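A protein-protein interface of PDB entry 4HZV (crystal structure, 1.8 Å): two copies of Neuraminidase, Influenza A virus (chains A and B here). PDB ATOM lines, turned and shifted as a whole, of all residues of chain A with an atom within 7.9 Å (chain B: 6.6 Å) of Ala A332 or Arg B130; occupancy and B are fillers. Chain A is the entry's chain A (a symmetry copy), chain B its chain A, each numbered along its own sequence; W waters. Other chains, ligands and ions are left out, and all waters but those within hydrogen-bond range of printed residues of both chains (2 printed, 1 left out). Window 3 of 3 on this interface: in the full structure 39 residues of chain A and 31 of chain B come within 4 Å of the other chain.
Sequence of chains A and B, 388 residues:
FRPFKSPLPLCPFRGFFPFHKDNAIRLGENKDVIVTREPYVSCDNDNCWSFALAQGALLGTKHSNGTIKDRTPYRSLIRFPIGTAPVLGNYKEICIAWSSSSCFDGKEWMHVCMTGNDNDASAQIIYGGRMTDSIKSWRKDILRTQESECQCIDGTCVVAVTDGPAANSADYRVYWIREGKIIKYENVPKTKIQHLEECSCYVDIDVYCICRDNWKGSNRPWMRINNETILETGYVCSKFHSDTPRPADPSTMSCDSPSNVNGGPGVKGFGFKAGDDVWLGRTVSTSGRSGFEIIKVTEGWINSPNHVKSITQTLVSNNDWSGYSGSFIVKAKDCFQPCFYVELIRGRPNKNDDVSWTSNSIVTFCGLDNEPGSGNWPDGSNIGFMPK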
ATOM      1  N   LEU A   8      27.111  -1.121   9.876  1.00  0.00           N
ATOM      2  CA  LEU A   8      27.225  -2.177   8.869  1.00  0.00           C
ATOM      3  C   LEU A   8      27.989  -1.725   7.626  1.00  0.00           C
ATOM      4  O   LEU A   8      27.967  -0.550   7.270  1.00  0.00           O
ATOM      5  CB  LEU A   8      25.833  -2.662   8.457  1.00  0.00           C
ATOM      6  CG  LEU A   8      24.929  -3.146   9.589  1.00  0.00           C
ATOM      7  CD1 LEU A   8      23.504  -3.404   9.079  1.00  0.00           C
ATOM      8  CD2 LEU A   8      25.508  -4.396  10.222  1.00  0.00           C
ATOM      9  N   PRO A   9      28.663  -2.668   6.956  1.00  0.00           N
ATOM     10  CA  PRO A   9      29.337  -2.374   5.692  1.00  0.00           C
ATOM     11  C   PRO A   9      28.310  -2.187   4.582  1.00  0.00           C
ATOM     12  O   PRO A   9      27.193  -2.686   4.696  1.00  0.00           O
ATOM     13  CB  PRO A   9      30.141  -3.646   5.431  1.00  0.00           C
ATOM     14  CG  PRO A   9      29.322  -4.723   6.092  1.00  0.00           C
ATOM     15  CD  PRO A   9      28.828  -4.079   7.350  1.00  0.00           C
ATOM     16  N   CYS A  11      26.524  -3.014   1.165  1.00  0.00           N
ATOM     17  CA  CYS A  11      26.319  -4.247   0.410  1.00  0.00           C
ATOM     18  C   CYS A  11      27.095  -4.210  -0.901  1.00  0.00           C
ATOM     19  O   CYS A  11      27.365  -3.138  -1.437  1.00  0.00           O
ATOM     20  CB  CYS A  11      24.834  -4.442   0.102  1.00  0.00           C
ATOM     21  SG  CYS A  11      23.774  -4.626   1.550  1.00  0.00           S
ATOM     22  N   PHE A  19      13.414   2.200  -8.609  1.00  0.00           N
ATOM     23  CA  PHE A  19      12.768   1.841  -7.349  1.00  0.00           C
ATOM     24  C   PHE A  19      11.364   2.447  -7.300  1.00  0.00           C
ATOM     25  O   PHE A  19      10.383   1.798  -7.691  1.00  0.00           O
ATOM     26  CB  PHE A  19      13.640   2.374  -6.203  1.00  0.00           C
ATOM     27  CG  PHE A  19      13.296   1.830  -4.835  1.00  0.00           C
ATOM     28  CD1 PHE A  19      12.601   0.644  -4.678  1.00  0.00           C
ATOM     29  CD2 PHE A  19      13.710   2.514  -3.699  1.00  0.00           C
ATOM     30  CE1 PHE A  19      12.303   0.158  -3.409  1.00  0.00           C
ATOM     31  CE2 PHE A  19      13.416   2.033  -2.431  1.00  0.00           C
ATOM     32  CZ  PHE A  19      12.716   0.855  -2.288  1.00  0.00           C
ATOM     33  N   HIS A  20      11.290   3.697  -6.837  1.00  0.00           N
ATOM     34  CA  HIS A  20      10.041   4.451  -6.707  1.00  0.00           C
ATOM     35  C   HIS A  20      10.089   5.712  -7.564  1.00  0.00           C
ATOM     36  O   HIS A  20      11.125   6.354  -7.657  1.00  0.00           O
ATOM     37  CB  HIS A  20       9.840   4.902  -5.254  1.00  0.00           C
ATOM     38  CG  HIS A  20       9.515   3.794  -4.299  1.00  0.00           C
ATOM     39  ND1 HIS A  20       8.225   3.360  -4.074  1.00  0.00           N
ATOM     40  CD2 HIS A  20      10.306   3.060  -3.482  1.00  0.00           C
ATOM     41  CE1 HIS A  20       8.238   2.393  -3.173  1.00  0.00           C
ATOM     42  NE2 HIS A  20       9.487   2.196  -2.792  1.00  0.00           N
ATOM     43  N   ASP A  46      10.155   0.396   9.293  1.00  0.00           N
ATOM     44  CA  ASP A  46       8.944  -0.083   8.632  1.00  0.00           C
ATOM     45  C   ASP A  46       8.731   0.474   7.224  1.00  0.00           C
ATOM     46  O   ASP A  46       8.151  -0.199   6.368  1.00  0.00           O
ATOM     47  CB  ASP A  46       7.729   0.214   9.508  1.00  0.00           C
ATOM     48  CG  ASP A  46       7.793  -0.498  10.847  1.00  0.00           C
ATOM     49  OD1 ASP A  46       8.055  -1.721  10.860  1.00  0.00           O
ATOM     50  OD2 ASP A  46       7.583   0.163  11.882  1.00  0.00           O
ATOM     51  N   CYS A  48      10.181   3.373   3.921  1.00  0.00           N
ATOM     52  CA  CYS A  48      10.971   4.454   3.354  1.00  0.00           C
ATOM     53  C   CYS A  48      10.016   5.612   3.106  1.00  0.00           C
ATOM     54  O   CYS A  48       8.841   5.392   2.793  1.00  0.00           O
ATOM     55  CB  CYS A  48      11.657   4.010   2.061  1.00  0.00           C
ATOM     56  SG  CYS A  48      13.116   2.986   2.356  1.00  0.00           S
ATOM     57  N   ILE A 329      20.356   4.899   2.498  1.00  0.00           N
ATOM     58  CA  ILE A 329      20.645   3.482   2.669  1.00  0.00           C
ATOM     59  C   ILE A 329      19.411   2.741   3.152  1.00  0.00           C
ATOM     60  O   ILE A 329      18.512   3.339   3.746  1.00  0.00           O
ATOM     61  CB  ILE A 329      21.773   3.247   3.688  1.00  0.00           C
ATOM     62  CG1 ILE A 329      21.418   3.902   5.025  1.00  0.00           C
ATOM     63  CG2 ILE A 329      23.109   3.759   3.152  1.00  0.00           C
ATOM     64  CD1 ILE A 329      22.465   3.688   6.104  1.00  0.00           C
ATOM     65  N   VAL A 330      19.378   1.438   2.888  1.00  0.00           N
ATOM     66  CA  VAL A 330      18.319   0.570   3.388  1.00  0.00           C
ATOM     67  C   VAL A 330      18.968  -0.657   4.015  1.00  0.00           C
ATOM     68  O   VAL A 330      19.803  -1.309   3.388  1.00  0.00           O
ATOM     69  CB  VAL A 330      17.376   0.120   2.260  1.00  0.00           C
ATOM     70  CG1 VAL A 330      16.272  -0.751   2.820  1.00  0.00           C
ATOM     71  CG2 VAL A 330      16.790   1.328   1.533  1.00  0.00           C
ATOM     72  N   LYS A 331      18.612  -0.961   5.257  1.00  0.00           N
ATOM     73  CA  LYS A 331      19.243  -2.085   5.935  1.00  0.00           C
ATOM     74  C   LYS A 331      18.879  -3.385   5.242  1.00  0.00           C
ATOM     75  O   LYS A 331      17.704  -3.667   5.012  1.00  0.00           O
ATOM     76  CB  LYS A 331      18.845  -2.158   7.405  1.00  0.00           C
ATOM     77  CG  LYS A 331      19.611  -3.233   8.161  1.00  0.00           C
ATOM     78  CD  LYS A 331      19.171  -3.341   9.612  1.00  0.00           C
ATOM     79  CE  LYS A 331      19.640  -4.660  10.207  1.00  0.00           C
ATOM     80  NZ  LYS A 331      19.059  -4.909  11.554  1.00  0.00           N
ATOM     81  N   ALA A 332      19.895  -4.172   4.919  1.00  0.00           N
ATOM     82  CA  ALA A 332      19.702  -5.426   4.201  1.00  0.00           C
ATOM     83  C   ALA A 332      20.356  -6.611   4.896  1.00  0.00           C
ATOM     84  O   ALA A 332      21.311  -7.186   4.378  1.00  0.00           O
ATOM     85  CB  ALA A 332      20.241  -5.302   2.786  1.00  0.00           C
ATOM     86  N   LYS A 333      19.838  -6.962   6.069  1.00  0.00           N
ATOM     87  CA  LYS A 333      20.395  -8.044   6.881  1.00  0.00           C
ATOM     88  C   LYS A 333      21.682  -7.341   7.307  1.00  0.00           C
ATOM     89  O   LYS A 333      21.647  -6.261   7.903  1.00  0.00           O
ATOM     90  CB  LYS A 333      20.672  -9.294   6.036  1.00  0.00           C
ATOM     91  CG  LYS A 333      19.503  -9.783   5.190  1.00  0.00           C
ATOM     92  CD  LYS A 333      18.397 -10.400   6.032  1.00  0.00           C
ATOM     93  CE  LYS A 333      17.330 -11.030   5.143  1.00  0.00           C
ATOM     94  NZ  LYS A 333      16.236 -11.664   5.928  1.00  0.00           N
ATOM     95  N   ASP A 334      22.818  -7.955   6.988  1.00  0.00           N
ATOM     96  CA  ASP A 334      24.116  -7.646   7.580  1.00  0.00           C
ATOM     97  C   ASP A 334      24.890  -6.585   6.799  1.00  0.00           C
ATOM     98  O   ASP A 334      26.073  -6.358   7.053  1.00  0.00           O
ATOM     99  CB  ASP A 334      24.952  -8.921   7.728  1.00  0.00           C
ATOM    100  CG  ASP A 334      24.883  -9.809   6.503  1.00  0.00           C
ATOM    101  OD1 ASP A 334      25.036 -11.041   6.656  1.00  0.00           O
ATOM    102  OD2 ASP A 334      24.667  -9.280   5.388  1.00  0.00           O
ATOM    103  N   CYS A 335      24.226  -5.937   5.849  1.00  0.00           N
ATOM    104  CA  CYS A 335      24.843  -4.834   5.123  1.00  0.00           C
ATOM    105  C   CYS A 335      23.828  -3.749   4.783  1.00  0.00           C
ATOM    106  O   CYS A 335      22.619  -3.964   4.876  1.00  0.00           O
ATOM    107  CB  CYS A 335      25.545  -5.329   3.857  1.00  0.00           C
ATOM    108  SG  CYS A 335      24.465  -6.174   2.671  1.00  0.00           S
ATOM    109  N   PHE A 336      24.332  -2.577   4.409  1.00  0.00           N
ATOM    110  CA  PHE A 336      23.480  -1.476   3.979  1.00  0.00           C
ATOM    111  C   PHE A 336      23.449  -1.404   2.461  1.00  0.00           C
ATOM    112  O   PHE A 336      24.490  -1.361   1.808  1.00  0.00           O
ATOM    113  CB  PHE A 336      23.987  -0.143   4.532  1.00  0.00           C
ATOM    114  CG  PHE A 336      23.656   0.076   5.981  1.00  0.00           C
ATOM    115  CD1 PHE A 336      22.344   0.013   6.421  1.00  0.00           C
ATOM    116  CD2 PHE A 336      24.654   0.368   6.900  1.00  0.00           C
ATOM    117  CE1 PHE A 336      22.030   0.215   7.756  1.00  0.00           C
ATOM    118  CE2 PHE A 336      24.346   0.580   8.242  1.00  0.00           C
ATOM    119  CZ  PHE A 336      23.031   0.504   8.669  1.00  0.00           C
ATOM    120  N   GLN A 337      22.246  -1.380   1.905  1.00  0.00           N
ATOM    121  CA  GLN A 337      22.082  -1.229   0.475  1.00  0.00           C
ATOM    122  C   GLN A 337      22.185   0.242   0.083  1.00  0.00           C
ATOM    123  O   GLN A 337      21.505   1.091   0.660  1.00  0.00           O
ATOM    124  CB  GLN A 337      20.729  -1.805   0.059  1.00  0.00           C
ATOM    125  CG  GLN A 337      20.390  -1.594  -1.390  1.00  0.00           C
ATOM    126  CD  GLN A 337      19.020  -2.116  -1.720  1.00  0.00           C
ATOM    127  OE1 GLN A 337      18.105  -2.043  -0.901  1.00  0.00           O
ATOM    128  NE2 GLN A 337      18.870  -2.660  -2.920  1.00  0.00           N
ATOM    129  N   PRO A 338      23.055   0.555  -0.893  1.00  0.00           N
ATOM    130  CA  PRO A 338      23.147   1.925  -1.407  1.00  0.00           C
ATOM    131  C   PRO A 338      22.015   2.238  -2.374  1.00  0.00           C
ATOM    132  O   PRO A 338      21.792   1.479  -3.326  1.00  0.00           O
ATOM    133  CB  PRO A 338      24.479   1.923  -2.156  1.00  0.00           C
ATOM    134  CG  PRO A 338      24.624   0.505  -2.625  1.00  0.00           C
ATOM    135  CD  PRO A 338      24.060  -0.333  -1.503  1.00  0.00           C
ATOM    136  N   CYS A 339      21.304   3.336  -2.116  1.00  0.00           N
ATOM    137  CA  CYS A 339      20.258   3.819  -3.008  1.00  0.00           C
ATOM    138  C   CYS A 339      20.450   5.312  -3.199  1.00  0.00           C
ATOM    139  O   CYS A 339      21.197   5.956  -2.452  1.00  0.00           O
ATOM    140  CB  CYS A 339      18.859   3.574  -2.414  1.00  0.00           C
ATOM    141  SG  CYS A 339      18.438   1.873  -2.020  1.00  0.00           S
ATOM    142  N   CYS A 366      18.027   1.825  -6.563  1.00  0.00           N
ATOM    143  CA  CYS A 366      18.825   1.126  -5.562  1.00  0.00           C
ATOM    144  C   CYS A 366      19.849   0.202  -6.199  1.00  0.00           C
ATOM    145  O   CYS A 366      19.648  -0.297  -7.312  1.00  0.00           O
ATOM    146  CB  CYS A 366      17.951   0.314  -4.613  1.00  0.00           C
ATOM    147  SG  CYS A 366      17.049   1.335  -3.421  1.00  0.00           S
ATOM    148  N   GLY A 367      20.927  -0.044  -5.465  1.00  0.00           N
ATOM    149  CA  GLY A 367      22.002  -0.893  -5.941  1.00  0.00           C
ATOM    150  C   GLY A 367      21.780  -2.368  -5.668  1.00  0.00           C
ATOM    151  O   GLY A 367      21.392  -2.760  -4.560  1.00  0.00           O
ATOM    152  N   LEU A 368      22.014  -3.190  -6.689  1.00  0.00           N
ATOM    153  CA  LEU A 368      21.989  -4.640  -6.531  1.00  0.00           C
ATOM    154  C   LEU A 368      23.247  -5.233  -7.155  1.00  0.00           C
ATOM    155  O   LEU A 368      23.862  -4.617  -8.018  1.00  0.00           O
ATOM    156  CB  LEU A 368      20.765  -5.252  -7.211  1.00  0.00           C
ATOM    157  CG  LEU A 368      19.385  -4.856  -6.696  1.00  0.00           C
ATOM    158  CD1 LEU A 368      18.315  -5.407  -7.650  1.00  0.00           C
ATOM    159  CD2 LEU A 368      19.181  -5.367  -5.280  1.00  0.00           C
ATOM    160  N   ILE B 125      12.662  -7.083  -7.691  1.00  0.00           N
ATOM    161  CA  ILE B 125      11.984  -7.845  -6.652  1.00  0.00           C
ATOM    162  C   ILE B 125      11.992  -7.018  -5.372  1.00  0.00           C
ATOM    163  O   ILE B 125      13.062  -6.628  -4.884  1.00  0.00           O
ATOM    164  CB  ILE B 125      12.678  -9.200  -6.398  1.00  0.00           C
ATOM    165  CG1 ILE B 125      12.859  -9.964  -7.711  1.00  0.00           C
ATOM    166  CG2 ILE B 125      11.887 -10.032  -5.409  1.00  0.00           C
ATOM    167  CD1 ILE B 125      11.550 -10.340  -8.388  1.00  0.00           C
ATOM    168  N   ILE B 126      10.801  -6.712  -4.860  1.00  0.00           N
ATOM    169  CA  ILE B 126      10.663  -5.957  -3.618  1.00  0.00           C
ATOM    170  C   ILE B 126      10.183  -6.907  -2.527  1.00  0.00           C
ATOM    171  O   ILE B 126       9.271  -7.702  -2.752  1.00  0.00           O
ATOM    172  CB  ILE B 126       9.627  -4.799  -3.742  1.00  0.00           C
ATOM    173  CG1 ILE B 126       9.829  -4.000  -5.037  1.00  0.00           C
ATOM    174  CG2 ILE B 126       9.706  -3.888  -2.524  1.00  0.00           C
ATOM    175  CD1 ILE B 126      11.200  -3.376  -5.178  1.00  0.00           C
ATOM    176  N   TYR B 127      10.797  -6.837  -1.348  1.00  0.00           N
ATOM    177  CA  TYR B 127      10.368  -7.673  -0.230  1.00  0.00           C
ATOM    178  C   TYR B 127      10.427  -6.863   1.061  1.00  0.00           C
ATOM    179  O   TYR B 127      11.483  -6.350   1.425  1.00  0.00           O
ATOM    180  CB  TYR B 127      11.221  -8.941  -0.106  1.00  0.00           C
ATOM    181  CG  TYR B 127      10.721  -9.897   0.964  1.00  0.00           C
ATOM    182  CD1 TYR B 127       9.618 -10.714   0.732  1.00  0.00           C
ATOM    183  CD2 TYR B 127      11.340  -9.972   2.208  1.00  0.00           C
ATOM    184  CE1 TYR B 127       9.146 -11.579   1.707  1.00  0.00           C
ATOM    185  CE2 TYR B 127      10.876 -10.837   3.188  1.00  0.00           C
ATOM    186  CZ  TYR B 127       9.782 -11.640   2.933  1.00  0.00           C
ATOM    187  OH  TYR B 127       9.318 -12.496   3.907  1.00  0.00           O
ATOM    188  N   GLY B 128       9.289  -6.740   1.738  1.00  0.00           N
ATOM    189  CA  GLY B 128       9.208  -5.927   2.942  1.00  0.00           C
ATOM    190  C   GLY B 128       9.611  -4.493   2.649  1.00  0.00           C
ATOM    191  O   GLY B 128      10.191  -3.802   3.497  1.00  0.00           O
ATOM    192  N   GLY B 129       9.324  -4.052   1.429  1.00  0.00           N
ATOM    193  CA  GLY B 129       9.594  -2.685   1.030  1.00  0.00           C
ATOM    194  C   GLY B 129      11.001  -2.440   0.521  1.00  0.00           C
ATOM    195  O   GLY B 129      11.304  -1.348   0.046  1.00  0.00           O
ATOM    196  N   ARG B 130      11.861  -3.448   0.619  1.00  0.00           N
ATOM    197  CA  ARG B 130      13.242  -3.308   0.157  1.00  0.00           C
ATOM    198  C   ARG B 130      13.465  -4.024  -1.162  1.00  0.00           C
ATOM    199  O   ARG B 130      12.999  -5.138  -1.341  1.00  0.00           O
ATOM    200  CB  ARG B 130      14.219  -3.863   1.191  1.00  0.00           C
ATOM    201  CG  ARG B 130      15.673  -3.655   0.796  1.00  0.00           C
ATOM    202  CD  ARG B 130      16.615  -4.052   1.916  1.00  0.00           C
ATOM    203  NE  ARG B 130      17.334  -5.274   1.592  1.00  0.00           N
ATOM    204  CZ  ARG B 130      17.027  -6.481   2.052  1.00  0.00           C
ATOM    205  NH1 ARG B 130      16.002  -6.647   2.881  1.00  0.00           N
ATOM    206  NH2 ARG B 130      17.756  -7.529   1.676  1.00  0.00           N
ATOM    207  N   MET B 131      14.189  -3.387  -2.076  1.00  0.00           N
ATOM    208  CA  MET B 131      14.566  -4.039  -3.327  1.00  0.00           C
ATOM    209  C   MET B 131      15.660  -5.066  -3.060  1.00  0.00           C
ATOM    210  O   MET B 131      16.786  -4.706  -2.723  1.00  0.00           O
ATOM    211  CB  MET B 131      15.055  -3.024  -4.361  1.00  0.00           C
ATOM    212  CG  MET B 131      15.316  -3.667  -5.729  1.00  0.00           C
ATOM    213  SD  MET B 131      16.125  -2.566  -6.899  1.00  0.00           S
ATOM    214  CE  MET B 131      15.038  -1.143  -6.861  1.00  0.00           C
ATOM    215  N   THR B 132      15.324  -6.337  -3.230  1.00  0.00           N
ATOM    216  CA  THR B 132      16.179  -7.440  -2.796  1.00  0.00           C
ATOM    217  C   THR B 132      16.858  -8.206  -3.926  1.00  0.00           C
ATOM    218  O   THR B 132      17.858  -8.886  -3.703  1.00  0.00           O
ATOM    219  CB  THR B 132      15.366  -8.459  -1.994  1.00  0.00           C
ATOM    220  OG1 THR B 132      14.171  -8.773  -2.719  1.00  0.00           O
ATOM    221  CG2 THR B 132      14.987  -7.895  -0.644  1.00  0.00           C
ATOM    222  N   ASP B 133      16.311  -8.123  -5.131  1.00  0.00           N
ATOM    223  CA  ASP B 133      16.852  -8.899  -6.245  1.00  0.00           C
ATOM    224  C   ASP B 133      16.285  -8.360  -7.553  1.00  0.00           C
ATOM    225  O   ASP B 133      15.502  -7.405  -7.553  1.00  0.00           O
ATOM    226  CB  ASP B 133      16.513 -10.385  -6.067  1.00  0.00           C
ATOM    227  CG  ASP B 133      17.628 -11.316  -6.552  1.00  0.00           C
ATOM    228  OD1 ASP B 133      18.429 -10.919  -7.428  1.00  0.00           O
ATOM    229  OD2 ASP B 133      17.689 -12.457  -6.049  1.00  0.00           O
ATOM    230  N   GLU B 179      12.003 -14.756   0.633  1.00  0.00           N
ATOM    231  CA  GLU B 179      12.369 -13.521   1.317  1.00  0.00           C
ATOM    232  C   GLU B 179      13.016 -12.528   0.350  1.00  0.00           C
ATOM    233  O   GLU B 179      13.968 -11.824   0.701  1.00  0.00           O
ATOM    234  CB  GLU B 179      13.289 -13.815   2.501  1.00  0.00           C
ATOM    235  CG  GLU B 179      12.679 -14.777   3.507  1.00  0.00           C
ATOM    236  CD  GLU B 179      13.668 -15.203   4.576  1.00  0.00           C
ATOM    237  OE1 GLU B 179      14.418 -14.336   5.065  1.00  0.00           O
ATOM    238  OE2 GLU B 179      13.698 -16.404   4.930  1.00  0.00           O
ATOM    239  N   GLY B 180      12.492 -12.486  -0.873  1.00  0.00           N
ATOM    240  CA  GLY B 180      12.923 -11.520  -1.866  1.00  0.00           C
ATOM    241  C   GLY B 180      14.132 -11.948  -2.673  1.00  0.00           C
ATOM    242  O   GLY B 180      14.562 -11.231  -3.581  1.00  0.00           O
ATOM    243  N   LYS B 181      14.681 -13.114  -2.347  1.00  0.00           N
ATOM    244  CA  LYS B 181      15.856 -13.613  -3.059  1.00  0.00           C
ATOM    245  C   LYS B 181      15.512 -14.761  -3.991  1.00  0.00           C
ATOM    246  O   LYS B 181      14.918 -15.769  -3.583  1.00  0.00           O
ATOM    247  CB  LYS B 181      16.963 -14.025  -2.087  1.00  0.00           C
ATOM    248  CG  LYS B 181      17.541 -12.868  -1.274  1.00  0.00           C
ATOM    249  CD  LYS B 181      17.997 -11.711  -2.172  1.00  0.00           C
ATOM    250  CE  LYS B 181      18.688 -10.604  -1.376  1.00  0.00           C
ATOM    251  NZ  LYS B 181      20.105 -10.938  -1.027  1.00  0.00           N
HETATM  252  O   HOH W   1      15.653  -1.037  -1.379  1.00  0.00           O
HETATM  253  O   HOH W   2       9.532   0.514  -0.633  1.00  0.00           O
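The side-chain sulfur (SG) of Cys A335 forms a disulfide with the side-chain sulfur (SG) of Cys A11 (2.0 Å). The backbone carbonyl oxygen of Asp B133 sits at hydrogen-bond distance from the backbone NH of Ile B125, at 2.9 Å. SG of Cys A339 forms a disulfide with SG of Cys A366, at 2.0 Å. The side-chain sulfur of Cys A11 is in hydrogen-bond range of the backbone NH of Gln A337, 3.6 Å away. The side-chain amide nitrogen (NE2) of Gln A337 lies within hydrogen-bond range of the backbone carbonyl oxygen (O) of Gly A367. The backbone carbonyl oxygen (O) of Ile B125 lies within hydrogen-bond range of the backbone NH (N) of Thr B132.
Phe A19 touches Gly B129 (CZ to O, 3.5 Å). Phe A19 touches Met B131. Arg B130 touches Val A330. CD of Arg B130 touches O of Lys A331, 3.3 Å away. Arg B130 touches Ala A332 (NE to CB, 3.1 Å). Gln A337 touches Arg B130 (OE1 to CG, 3.4 Å). Cys A366 touches Met B131. Met B131 touches Leu A368. Thr B132 touches Leu A368. Asp B133 touches Leu A368.
No position is printed for both chains.
NZ of Lys A333 lies within salt-bridge range of OE1 of Glu B179 (3.3 Å). The side-chain amide nitrogen (NE2) of Gln A337 is in hydrogen-bond range of the backbone carbonyl oxygen (O) of Met B131, at 2.9 Å.
Water W2 bridges O of Gly B129 and NE2 of His A20. Water W1 lies within hydrogen-bond range of the side-chain amide oxygen of Gln A337, the backbone NH of Met B131 and the side-chain sulfur of Cys A366.
Printed residues of chain A that touch a printed residue of chain B: Phe A19, Val A330, Lys A331, Ala A332, Lys A333, Gln A337, Cys A366 and Leu A368. Hydrophobic or aromatic side chains of chain A that line the printed part of chain B: Phe A19, Val A330, Ala A332 and Leu A368. Of the 12 printed residues of chain B, 6 touch a printed residue of chain A. Hydrophobic or aromatic side chains of chain B that line the printed part of chain A: Met B131. Among the printed residues, Asp or Glu carboxylates within 4 Å of a Lys or Arg side-chain nitrogen of the other chain: Lys A333 with Glu B179 (3.3 Å).
Of the printed residues of chain B, Ala A332 touches Arg B130. Printed residues of chain A within 4 Å of Arg B130: Val A330 (3.4 Å), Lys A331 (3.3 Å), Ala A332 (3.1 Å) and Gln A337 (3.4 Å). Gly B129 touches just one residue of chain A: Phe A19. Of the printed residues of chain B, Leu A368 touches Met B131, Thr B132 and Asp B133. Of the printed residues of chain B, Phe A19 touches Gly B129 (3.5 Å) and Met B131 (3.7 Å). Printed residues of chain B within 4 Å of Cys A366: Met B131. Of the printed residues of chain A, Glu B179 touches Lys A333 (3.3 Å).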
